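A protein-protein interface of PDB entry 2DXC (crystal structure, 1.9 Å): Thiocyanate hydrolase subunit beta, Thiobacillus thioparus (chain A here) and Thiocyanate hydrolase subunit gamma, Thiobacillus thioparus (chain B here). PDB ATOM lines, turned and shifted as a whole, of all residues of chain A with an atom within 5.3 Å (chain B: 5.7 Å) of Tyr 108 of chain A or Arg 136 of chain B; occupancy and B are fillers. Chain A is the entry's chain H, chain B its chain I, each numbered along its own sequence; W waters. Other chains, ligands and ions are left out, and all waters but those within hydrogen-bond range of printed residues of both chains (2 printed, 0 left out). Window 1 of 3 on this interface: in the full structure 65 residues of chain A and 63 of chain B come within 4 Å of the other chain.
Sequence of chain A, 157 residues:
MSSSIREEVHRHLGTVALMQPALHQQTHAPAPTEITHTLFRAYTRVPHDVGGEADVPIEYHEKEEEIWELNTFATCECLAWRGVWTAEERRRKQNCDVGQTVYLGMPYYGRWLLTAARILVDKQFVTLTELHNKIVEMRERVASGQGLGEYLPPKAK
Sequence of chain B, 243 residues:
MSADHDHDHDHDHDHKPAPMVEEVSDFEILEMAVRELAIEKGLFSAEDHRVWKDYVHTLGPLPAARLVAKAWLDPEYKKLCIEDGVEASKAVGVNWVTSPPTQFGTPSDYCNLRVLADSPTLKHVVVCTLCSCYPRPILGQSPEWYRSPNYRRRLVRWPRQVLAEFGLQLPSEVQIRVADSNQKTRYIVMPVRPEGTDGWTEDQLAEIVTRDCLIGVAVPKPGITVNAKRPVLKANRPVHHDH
OH of Tyr 108 of chain A is in hydrogen-bond range of OG of Ser 132 of chain B (2.6 Å).
OG of Ser 142 of chain B sits at hydrogen-bond distance from NE of Arg 147 of chain B (2.9 Å). The guanidinium group (NH1) of Arg 136 of chain B lies within salt-bridge range of the side-chain carboxylate (OD1) of Asp 109 of chain B, at 2.8 Å. NH1 of Arg 147 of chain B is in salt-bridge range of OE1 of Glu 144 of chain B, at 3.7 Å.
CZ of Phe 73 of chain A touches NE of Arg 136 of chain B (3.4 Å). Tyr 108 of chain A touches Arg 136 of chain B. Arg 147 of chain B touches Tyr 108 of chain A (CD to CZ, 3.6 Å). CE2 of Tyr 109 of chain A touches NH1 of Arg 147 of chain B, 3.5 Å away.
Met 106 of chain A touches none of the printed residues of chain B. Printed residues of chain B within 4 Å of Tyr 108 of chain A: Ser 132, Arg 136 and Arg 147. Of the printed residues of chain B, Tyr 109 of chain A touches Arg 147. Pro 135 of chain B touches none of the printed residues of chain A. Printed residues of chain A within 4 Å of Arg 136 of chain B: Phe 73 and Tyr 108. Printed residues of chain A within 4 Å of Arg 147 of chain B: Tyr 108 and Tyr 109. The nearest printed residue of chain B that does not touch Tyr 108 of chain A is Ser 142 of chain B (4.5 Å). The nearest printed residue of chain A that does not touch Arg 136 of chain B is Trp 112 of chain A (4.04 Å). The nearest printed residue of chain B that does not touch Phe 73 of chain A is Gln 141 of chain B (5.1 Å).
Of the 8 printed residues of chain A, 3 touch a printed residue of chain B. Hydrophobic or aromatic side chains of chain A within 4 Å of the printed part of chain B: Phe 73, Tyr 108 and Tyr 109. Along chain A the printed residues that touch a printed residue of chain B span positions 73 to 109. Among the printed residues, no Asp or Glu carboxylate lies within 4 Å of a Lys or Arg side-chain nitrogen of the other chain.
Water W1 bridges OH of Tyr 109 of chain A and NE2 of Gln 141 of chain B. Water W2 lies within hydrogen-bond range of the side-chain hydroxyl (OH) of Tyr 109 of chain A (2.8 Å), the side-chain hydroxyl (OH) of Tyr 108 of chain A (2.9 Å) and the guanidinium group (NH2) of Arg 136 of chain B (3.0 Å).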
ATOM      1  N   PHE A  73      17.090  -8.979  25.642  1.00  0.00           N
ATOM      2  CA  PHE A  73      15.942  -8.925  24.744  1.00  0.00           C
ATOM      3  C   PHE A  73      16.325  -9.502  23.383  1.00  0.00           C
ATOM      4  O   PHE A  73      15.609 -10.337  22.832  1.00  0.00           O
ATOM      5  CB  PHE A  73      15.459  -7.482  24.577  1.00  0.00           C
ATOM      6  CG  PHE A  73      14.229  -7.352  23.722  1.00  0.00           C
ATOM      7  CD1 PHE A  73      13.033  -7.947  24.110  1.00  0.00           C
ATOM      8  CD2 PHE A  73      14.274  -6.671  22.512  1.00  0.00           C
ATOM      9  CE1 PHE A  73      11.900  -7.870  23.306  1.00  0.00           C
ATOM     10  CE2 PHE A  73      13.143  -6.589  21.698  1.00  0.00           C
ATOM     11  CZ  PHE A  73      11.955  -7.190  22.096  1.00  0.00           C
ATOM     12  N   MET A 106      11.994 -10.555  41.701  1.00  0.00           N
ATOM     13  CA  MET A 106      13.083 -10.225  40.781  1.00  0.00           C
ATOM     14  C   MET A 106      12.641  -9.231  39.710  1.00  0.00           C
ATOM     15  O   MET A 106      11.445  -9.032  39.494  1.00  0.00           O
ATOM     16  CB  MET A 106      13.599 -11.506  40.122  1.00  0.00           C
ATOM     17  CG  MET A 106      14.436 -12.382  41.052  1.00  0.00           C
ATOM     18  SD  MET A 106      16.108 -11.713  41.306  1.00  0.00           S
ATOM     19  CE  MET A 106      16.923 -12.401  39.837  1.00  0.00           C
ATOM     20  N   PRO A 107      13.607  -8.594  39.022  1.00  0.00           N
ATOM     21  CA  PRO A 107      13.293  -7.618  37.974  1.00  0.00           C
ATOM     22  C   PRO A 107      12.751  -8.251  36.700  1.00  0.00           C
ATOM     23  O   PRO A 107      13.060  -9.399  36.377  1.00  0.00           O
ATOM     24  CB  PRO A 107      14.636  -6.928  37.709  1.00  0.00           C
ATOM     25  CG  PRO A 107      15.450  -7.210  38.945  1.00  0.00           C
ATOM     26  CD  PRO A 107      15.057  -8.630  39.267  1.00  0.00           C
ATOM     27  N   TYR A 108      11.952  -7.462  35.990  1.00  0.00           N
ATOM     28  CA  TYR A 108      11.338  -7.826  34.718  1.00  0.00           C
ATOM     29  C   TYR A 108      12.347  -8.542  33.810  1.00  0.00           C
ATOM     30  O   TYR A 108      12.176  -9.716  33.485  1.00  0.00           O
ATOM     31  CB  TYR A 108      10.832  -6.536  34.057  1.00  0.00           C
ATOM     32  CG  TYR A 108      10.318  -6.638  32.636  1.00  0.00           C
ATOM     33  CD1 TYR A 108       8.990  -6.981  32.368  1.00  0.00           C
ATOM     34  CD2 TYR A 108      11.140  -6.305  31.560  1.00  0.00           C
ATOM     35  CE1 TYR A 108       8.492  -6.977  31.063  1.00  0.00           C
ATOM     36  CE2 TYR A 108      10.655  -6.300  30.254  1.00  0.00           C
ATOM     37  CZ  TYR A 108       9.330  -6.632  30.013  1.00  0.00           C
ATOM     38  OH  TYR A 108       8.851  -6.586  28.724  1.00  0.00           O
ATOM     39  N   TYR A 109      13.402  -7.841  33.408  1.00  0.00           N
ATOM     40  CA  TYR A 109      14.395  -8.449  32.533  1.00  0.00           C
ATOM     41  C   TYR A 109      15.234  -9.534  33.198  1.00  0.00           C
ATOM     42  O   TYR A 109      15.890 -10.325  32.511  1.00  0.00           O
ATOM     43  CB  TYR A 109      15.295  -7.380  31.911  1.00  0.00           C
ATOM     44  CG  TYR A 109      14.782  -6.916  30.565  1.00  0.00           C
ATOM     45  CD1 TYR A 109      14.519  -7.838  29.551  1.00  0.00           C
ATOM     46  CD2 TYR A 109      14.543  -5.569  30.305  1.00  0.00           C
ATOM     47  CE1 TYR A 109      14.024  -7.434  28.317  1.00  0.00           C
ATOM     48  CE2 TYR A 109      14.049  -5.151  29.066  1.00  0.00           C
ATOM     49  CZ  TYR A 109      13.792  -6.090  28.080  1.00  0.00           C
ATOM     50  OH  TYR A 109      13.307  -5.692  26.857  1.00  0.00           O
ATOM     51  N   GLY A 110      15.215  -9.575  34.527  1.00  0.00           N
ATOM     52  CA  GLY A 110      15.955 -10.611  35.226  1.00  0.00           C
ATOM     53  C   GLY A 110      15.300 -11.946  34.912  1.00  0.00           C
ATOM     54  O   GLY A 110      15.975 -12.963  34.738  1.00  0.00           O
ATOM     55  N   ARG A 111      13.973 -11.939  34.824  1.00  0.00           N
ATOM     56  CA  ARG A 111      13.225 -13.152  34.525  1.00  0.00           C
ATOM     57  C   ARG A 111      13.419 -13.543  33.064  1.00  0.00           C
ATOM     58  O   ARG A 111      13.467 -14.726  32.735  1.00  0.00           O
ATOM     59  CB  ARG A 111      11.736 -12.950  34.838  1.00  0.00           C
ATOM     60  CG  ARG A 111      11.479 -12.656  36.310  1.00  0.00           C
ATOM     61  CD  ARG A 111       9.992 -12.540  36.658  1.00  0.00           C
ATOM     62  NE  ARG A 111       9.345 -11.405  36.008  1.00  0.00           N
ATOM     63  CZ  ARG A 111       8.670 -11.473  34.864  1.00  0.00           C
ATOM     64  NH1 ARG A 111       8.541 -12.628  34.225  1.00  0.00           N
ATOM     65  NH2 ARG A 111       8.109 -10.381  34.363  1.00  0.00           N
ATOM     66  N   TRP A 112      13.529 -12.547  32.188  1.00  0.00           N
ATOM     67  CA  TRP A 112      13.758 -12.822  30.776  1.00  0.00           C
ATOM     68  C   TRP A 112      15.082 -13.569  30.621  1.00  0.00           C
ATOM     69  O   TRP A 112      15.167 -14.580  29.926  1.00  0.00           O
ATOM     70  CB  TRP A 112      13.873 -11.525  29.974  1.00  0.00           C
ATOM     71  CG  TRP A 112      12.596 -10.892  29.559  1.00  0.00           C
ATOM     72  CD1 TRP A 112      11.689 -10.250  30.355  1.00  0.00           C
ATOM     73  CD2 TRP A 112      12.134 -10.737  28.216  1.00  0.00           C
ATOM     74  NE1 TRP A 112      10.698  -9.692  29.583  1.00  0.00           N
ATOM     75  CE2 TRP A 112      10.952  -9.978  28.265  1.00  0.00           C
ATOM     76  CE3 TRP A 112      12.613 -11.162  26.969  1.00  0.00           C
ATOM     77  CZ2 TRP A 112      10.241  -9.633  27.112  1.00  0.00           C
ATOM     78  CZ3 TRP A 112      11.903 -10.819  25.823  1.00  0.00           C
ATOM     79  CH2 TRP A 112      10.731 -10.061  25.906  1.00  0.00           C
ATOM     80  N   TYR B  55      18.148  -3.593  14.704  1.00  0.00           N
ATOM     81  CA  TYR B  55      16.753  -3.447  14.304  1.00  0.00           C
ATOM     82  C   TYR B  55      15.997  -2.718  15.416  1.00  0.00           C
ATOM     83  O   TYR B  55      15.258  -1.767  15.158  1.00  0.00           O
ATOM     84  CB  TYR B  55      16.108  -4.813  14.064  1.00  0.00           C
ATOM     85  CG  TYR B  55      14.599  -4.751  13.928  1.00  0.00           C
ATOM     86  CD1 TYR B  55      13.999  -4.011  12.905  1.00  0.00           C
ATOM     87  CD2 TYR B  55      13.768  -5.417  14.834  1.00  0.00           C
ATOM     88  CE1 TYR B  55      12.608  -3.931  12.790  1.00  0.00           C
ATOM     89  CE2 TYR B  55      12.373  -5.344  14.726  1.00  0.00           C
ATOM     90  CZ  TYR B  55      11.804  -4.599  13.704  1.00  0.00           C
ATOM     91  OH  TYR B  55      10.432  -4.502  13.605  1.00  0.00           O
ATOM     92  N   LEU B  59      13.695   1.256  16.012  1.00  0.00           N
ATOM     93  CA  LEU B  59      12.307   1.362  16.437  1.00  0.00           C
ATOM     94  C   LEU B  59      12.046   2.598  17.289  1.00  0.00           C
ATOM     95  O   LEU B  59      12.928   3.086  17.992  1.00  0.00           O
ATOM     96  CB  LEU B  59      11.897   0.102  17.206  1.00  0.00           C
ATOM     97  CG  LEU B  59      12.095  -1.214  16.441  1.00  0.00           C
ATOM     98  CD1 LEU B  59      11.511  -2.365  17.246  1.00  0.00           C
ATOM     99  CD2 LEU B  59      11.418  -1.127  15.072  1.00  0.00           C
ATOM    100  N   GLY B  60      10.818   3.095  17.215  1.00  0.00           N
ATOM    101  CA  GLY B  60      10.428   4.277  17.960  1.00  0.00           C
ATOM    102  C   GLY B  60       8.963   4.574  17.694  1.00  0.00           C
ATOM    103  O   GLY B  60       8.320   3.839  16.939  1.00  0.00           O
ATOM    104  N   TRP B  96       4.774  -5.319   9.152  1.00  0.00           N
ATOM    105  CA  TRP B  96       4.853  -6.250  10.268  1.00  0.00           C
ATOM    106  C   TRP B  96       5.408  -7.623   9.933  1.00  0.00           C
ATOM    107  O   TRP B  96       5.885  -8.332  10.817  1.00  0.00           O
ATOM    108  CB  TRP B  96       3.481  -6.368  10.937  1.00  0.00           C
ATOM    109  CG  TRP B  96       3.139  -5.128  11.707  1.00  0.00           C
ATOM    110  CD1 TRP B  96       2.989  -3.865  11.205  1.00  0.00           C
ATOM    111  CD2 TRP B  96       2.993  -5.014  13.126  1.00  0.00           C
ATOM    112  NE1 TRP B  96       2.766  -2.969  12.225  1.00  0.00           N
ATOM    113  CE2 TRP B  96       2.764  -3.650  13.416  1.00  0.00           C
ATOM    114  CE3 TRP B  96       3.036  -5.933  14.183  1.00  0.00           C
ATOM    115  CZ2 TRP B  96       2.578  -3.182  14.719  1.00  0.00           C
ATOM    116  CZ3 TRP B  96       2.851  -5.468  15.480  1.00  0.00           C
ATOM    117  CH2 TRP B  96       2.626  -4.103  15.736  1.00  0.00           C
ATOM    118  N   SER B 108       7.837 -12.120  19.145  1.00  0.00           N
ATOM    119  CA  SER B 108       6.990 -11.708  20.267  1.00  0.00           C
ATOM    120  C   SER B 108       5.861 -10.705  20.014  1.00  0.00           C
ATOM    121  O   SER B 108       4.928 -10.619  20.816  1.00  0.00           O
ATOM    122  CB  SER B 108       7.873 -11.179  21.402  1.00  0.00           C
ATOM    123  OG  SER B 108       8.785 -12.173  21.844  1.00  0.00           O
ATOM    124  N   ASP B 109       5.931  -9.946  18.923  1.00  0.00           N
ATOM    125  CA  ASP B 109       4.883  -8.960  18.644  1.00  0.00           C
ATOM    126  C   ASP B 109       3.872  -9.447  17.604  1.00  0.00           C
ATOM    127  O   ASP B 109       2.796  -8.865  17.449  1.00  0.00           O
ATOM    128  CB  ASP B 109       5.510  -7.643  18.176  1.00  0.00           C
ATOM    129  CG  ASP B 109       6.674  -7.211  19.048  1.00  0.00           C
ATOM    130  OD1 ASP B 109       6.477  -7.006  20.266  1.00  0.00           O
ATOM    131  OD2 ASP B 109       7.794  -7.082  18.508  1.00  0.00           O
ATOM    132  N   CSD B 131       1.445  -9.497  30.926  1.00  0.00           N
ATOM    133  CA  CSD B 131       2.851  -9.156  30.787  1.00  0.00           C
ATOM    134  CB  CSD B 131       3.665 -10.234  30.071  1.00  0.00           C
ATOM    135  SG  CSD B 131       2.965 -10.697  28.446  1.00  0.00           S
ATOM    136  C   CSD B 131       3.226  -7.746  30.341  1.00  0.00           C
ATOM    137  O   CSD B 131       3.207  -6.810  31.138  1.00  0.00           O
ATOM    138  OD1 CSD B 131       1.723 -11.357  28.634  1.00  0.00           O
ATOM    139  OD2 CSD B 131       3.906 -11.622  27.743  1.00  0.00           O
ATOM    140  N   SER B 132       3.568  -7.590  29.069  1.00  0.00           N
ATOM    141  CA  SER B 132       3.931  -6.272  28.569  1.00  0.00           C
ATOM    142  C   SER B 132       3.757  -6.148  27.068  1.00  0.00           C
ATOM    143  O   SER B 132       4.333  -5.251  26.447  1.00  0.00           O
ATOM    144  CB  SER B 132       5.371  -5.925  28.960  1.00  0.00           C
ATOM    145  OG  SER B 132       6.280  -6.929  28.541  1.00  0.00           O
ATOM    146  N   TYR B 134       3.320  -5.231  23.529  1.00  0.00           N
ATOM    147  CA  TYR B 134       3.375  -3.869  23.000  1.00  0.00           C
ATOM    148  C   TYR B 134       3.649  -3.925  21.492  1.00  0.00           C
ATOM    149  O   TYR B 134       4.359  -4.814  21.026  1.00  0.00           O
ATOM    150  CB  TYR B 134       4.534  -3.179  23.726  1.00  0.00           C
ATOM    151  CG  TYR B 134       4.617  -1.676  23.675  1.00  0.00           C
ATOM    152  CD1 TYR B 134       3.760  -0.882  24.435  1.00  0.00           C
ATOM    153  CD2 TYR B 134       5.632  -1.047  22.952  1.00  0.00           C
ATOM    154  CE1 TYR B 134       3.919   0.506  24.488  1.00  0.00           C
ATOM    155  CE2 TYR B 134       5.799   0.335  22.996  1.00  0.00           C
ATOM    156  CZ  TYR B 134       4.943   1.107  23.770  1.00  0.00           C
ATOM    157  OH  TYR B 134       5.129   2.472  23.838  1.00  0.00           O
ATOM    158  N   PRO B 135       3.099  -2.973  20.712  1.00  0.00           N
ATOM    159  CA  PRO B 135       3.297  -2.936  19.254  1.00  0.00           C
ATOM    160  C   PRO B 135       4.690  -2.434  18.869  1.00  0.00           C
ATOM    161  O   PRO B 135       4.825  -1.462  18.122  1.00  0.00           O
ATOM    162  CB  PRO B 135       2.193  -1.993  18.790  1.00  0.00           C
ATOM    163  CG  PRO B 135       2.141  -0.986  19.914  1.00  0.00           C
ATOM    164  CD  PRO B 135       2.204  -1.880  21.150  1.00  0.00           C
ATOM    165  N   ARG B 136       5.718  -3.118  19.368  1.00  0.00           N
ATOM    166  CA  ARG B 136       7.102  -2.724  19.134  1.00  0.00           C
ATOM    167  C   ARG B 136       7.497  -2.309  17.710  1.00  0.00           C
ATOM    168  O   ARG B 136       8.110  -1.258  17.521  1.00  0.00           O
ATOM    169  CB  ARG B 136       8.055  -3.826  19.620  1.00  0.00           C
ATOM    170  CG  ARG B 136       7.972  -4.140  21.119  1.00  0.00           C
ATOM    171  CD  ARG B 136       9.165  -5.005  21.544  1.00  0.00           C
ATOM    172  NE  ARG B 136       9.154  -5.392  22.958  1.00  0.00           N
ATOM    173  CZ  ARG B 136       8.581  -6.493  23.438  1.00  0.00           C
ATOM    174  NH1 ARG B 136       7.956  -7.336  22.622  1.00  0.00           N
ATOM    175  NH2 ARG B 136       8.655  -6.770  24.736  1.00  0.00           N
ATOM    176  N   PRO B 137       7.148  -3.113  16.692  1.00  0.00           N
ATOM    177  CA  PRO B 137       7.522  -2.744  15.321  1.00  0.00           C
ATOM    178  C   PRO B 137       7.183  -1.313  14.907  1.00  0.00           C
ATOM    179  O   PRO B 137       7.959  -0.666  14.205  1.00  0.00           O
ATOM    180  CB  PRO B 137       6.781  -3.772  14.467  1.00  0.00           C
ATOM    181  CG  PRO B 137       6.729  -4.982  15.367  1.00  0.00           C
ATOM    182  CD  PRO B 137       6.373  -4.368  16.707  1.00  0.00           C
ATOM    183  N   ILE B 138       6.036  -0.810  15.353  1.00  0.00           N
ATOM    184  CA  ILE B 138       5.609   0.534  14.976  1.00  0.00           C
ATOM    185  C   ILE B 138       5.677   1.583  16.085  1.00  0.00           C
ATOM    186  O   ILE B 138       5.530   2.771  15.810  1.00  0.00           O
ATOM    187  CB  ILE B 138       4.153   0.502  14.438  1.00  0.00           C
ATOM    188  CG1 ILE B 138       3.868   1.753  13.604  1.00  0.00           C
ATOM    189  CG2 ILE B 138       3.168   0.412  15.606  1.00  0.00           C
ATOM    190  CD1 ILE B 138       2.530   1.722  12.873  1.00  0.00           C
ATOM    191  N   LEU B 139       5.918   1.158  17.323  1.00  0.00           N
ATOM    192  CA  LEU B 139       5.940   2.098  18.445  1.00  0.00           C
ATOM    193  C   LEU B 139       7.236   2.131  19.258  1.00  0.00           C
ATOM    194  O   LEU B 139       7.493   3.088  19.985  1.00  0.00           O
ATOM    195  CB  LEU B 139       4.756   1.789  19.372  1.00  0.00           C
ATOM    196  CG  LEU B 139       4.420   2.741  20.527  1.00  0.00           C
ATOM    197  CD1 LEU B 139       4.215   4.159  19.997  1.00  0.00           C
ATOM    198  CD2 LEU B 139       3.155   2.251  21.229  1.00  0.00           C
ATOM    199  N   GLY B 140       8.052   1.089  19.142  1.00  0.00           N
ATOM    200  CA  GLY B 140       9.293   1.060  19.895  1.00  0.00           C
ATOM    201  C   GLY B 140       9.165   0.194  21.132  1.00  0.00           C
ATOM    202  O   GLY B 140       8.266  -0.648  21.212  1.00  0.00           O
ATOM    203  N   GLN B 141      10.051   0.394  22.104  1.00  0.00           N
ATOM    204  CA  GLN B 141      10.006  -0.401  23.326  1.00  0.00           C
ATOM    205  C   GLN B 141       9.003   0.155  24.329  1.00  0.00           C
ATOM    206  O   GLN B 141       8.741   1.357  24.365  1.00  0.00           O
ATOM    207  CB  GLN B 141      11.391  -0.476  23.966  1.00  0.00           C
ATOM    208  CG  GLN B 141      12.472  -0.960  23.014  1.00  0.00           C
ATOM    209  CD  GLN B 141      13.736  -1.383  23.736  1.00  0.00           C
ATOM    210  OE1 GLN B 141      14.849  -0.991  23.368  1.00  0.00           O
ATOM    211  NE2 GLN B 141      13.570  -2.201  24.772  1.00  0.00           N
ATOM    212  N   SER B 142       8.452  -0.733  25.148  1.00  0.00           N
ATOM    213  CA  SER B 142       7.461  -0.362  26.150  1.00  0.00           C
ATOM    214  C   SER B 142       8.056   0.428  27.312  1.00  0.00           C
ATOM    215  O   SER B 142       9.216   0.239  27.673  1.00  0.00           O
ATOM    216  CB  SER B 142       6.790  -1.624  26.690  1.00  0.00           C
ATOM    217  OG  SER B 142       7.750  -2.468  27.299  1.00  0.00           O
ATOM    218  N   GLU B 144       8.737   1.648  31.189  1.00  0.00           N
ATOM    219  CA  GLU B 144       8.950   0.861  32.400  1.00  0.00           C
ATOM    220  C   GLU B 144       7.634   0.679  33.161  1.00  0.00           C
ATOM    221  O   GLU B 144       7.309  -0.428  33.596  1.00  0.00           O
ATOM    222  CB  GLU B 144       9.981   1.545  33.310  1.00  0.00           C
ATOM    223  CG  GLU B 144      10.299   0.789  34.608  1.00  0.00           C
ATOM    224  CD  GLU B 144      11.190  -0.430  34.391  1.00  0.00           C
ATOM    225  OE1 GLU B 144      11.542  -0.714  33.226  1.00  0.00           O
ATOM    226  OE2 GLU B 144      11.543  -1.102  35.382  1.00  0.00           O
ATOM    227  N   ARG B 147       5.079  -1.982  32.051  1.00  0.00           N
ATOM    228  CA  ARG B 147       5.446  -3.344  32.438  1.00  0.00           C
ATOM    229  C   ARG B 147       5.170  -3.632  33.913  1.00  0.00           C
ATOM    230  O   ARG B 147       5.196  -4.794  34.339  1.00  0.00           O
ATOM    231  CB  ARG B 147       6.942  -3.566  32.204  1.00  0.00           C
ATOM    232  CG  ARG B 147       7.463  -3.118  30.848  1.00  0.00           C
ATOM    233  CD  ARG B 147       8.992  -3.102  30.828  1.00  0.00           C
ATOM    234  NE  ARG B 147       9.510  -2.679  29.531  1.00  0.00           N
ATOM    235  CZ  ARG B 147      10.800  -2.524  29.245  1.00  0.00           C
ATOM    236  NH1 ARG B 147      11.725  -2.755  30.167  1.00  0.00           N
ATOM    237  NH2 ARG B 147      11.164  -2.133  28.030  1.00  0.00           N
HETATM  238  O   HOH W   1      15.014  -3.913  26.229  1.00  0.00           O
HETATM  239  O   HOH W   2      10.540  -5.423  26.630  1.00  0.00           O
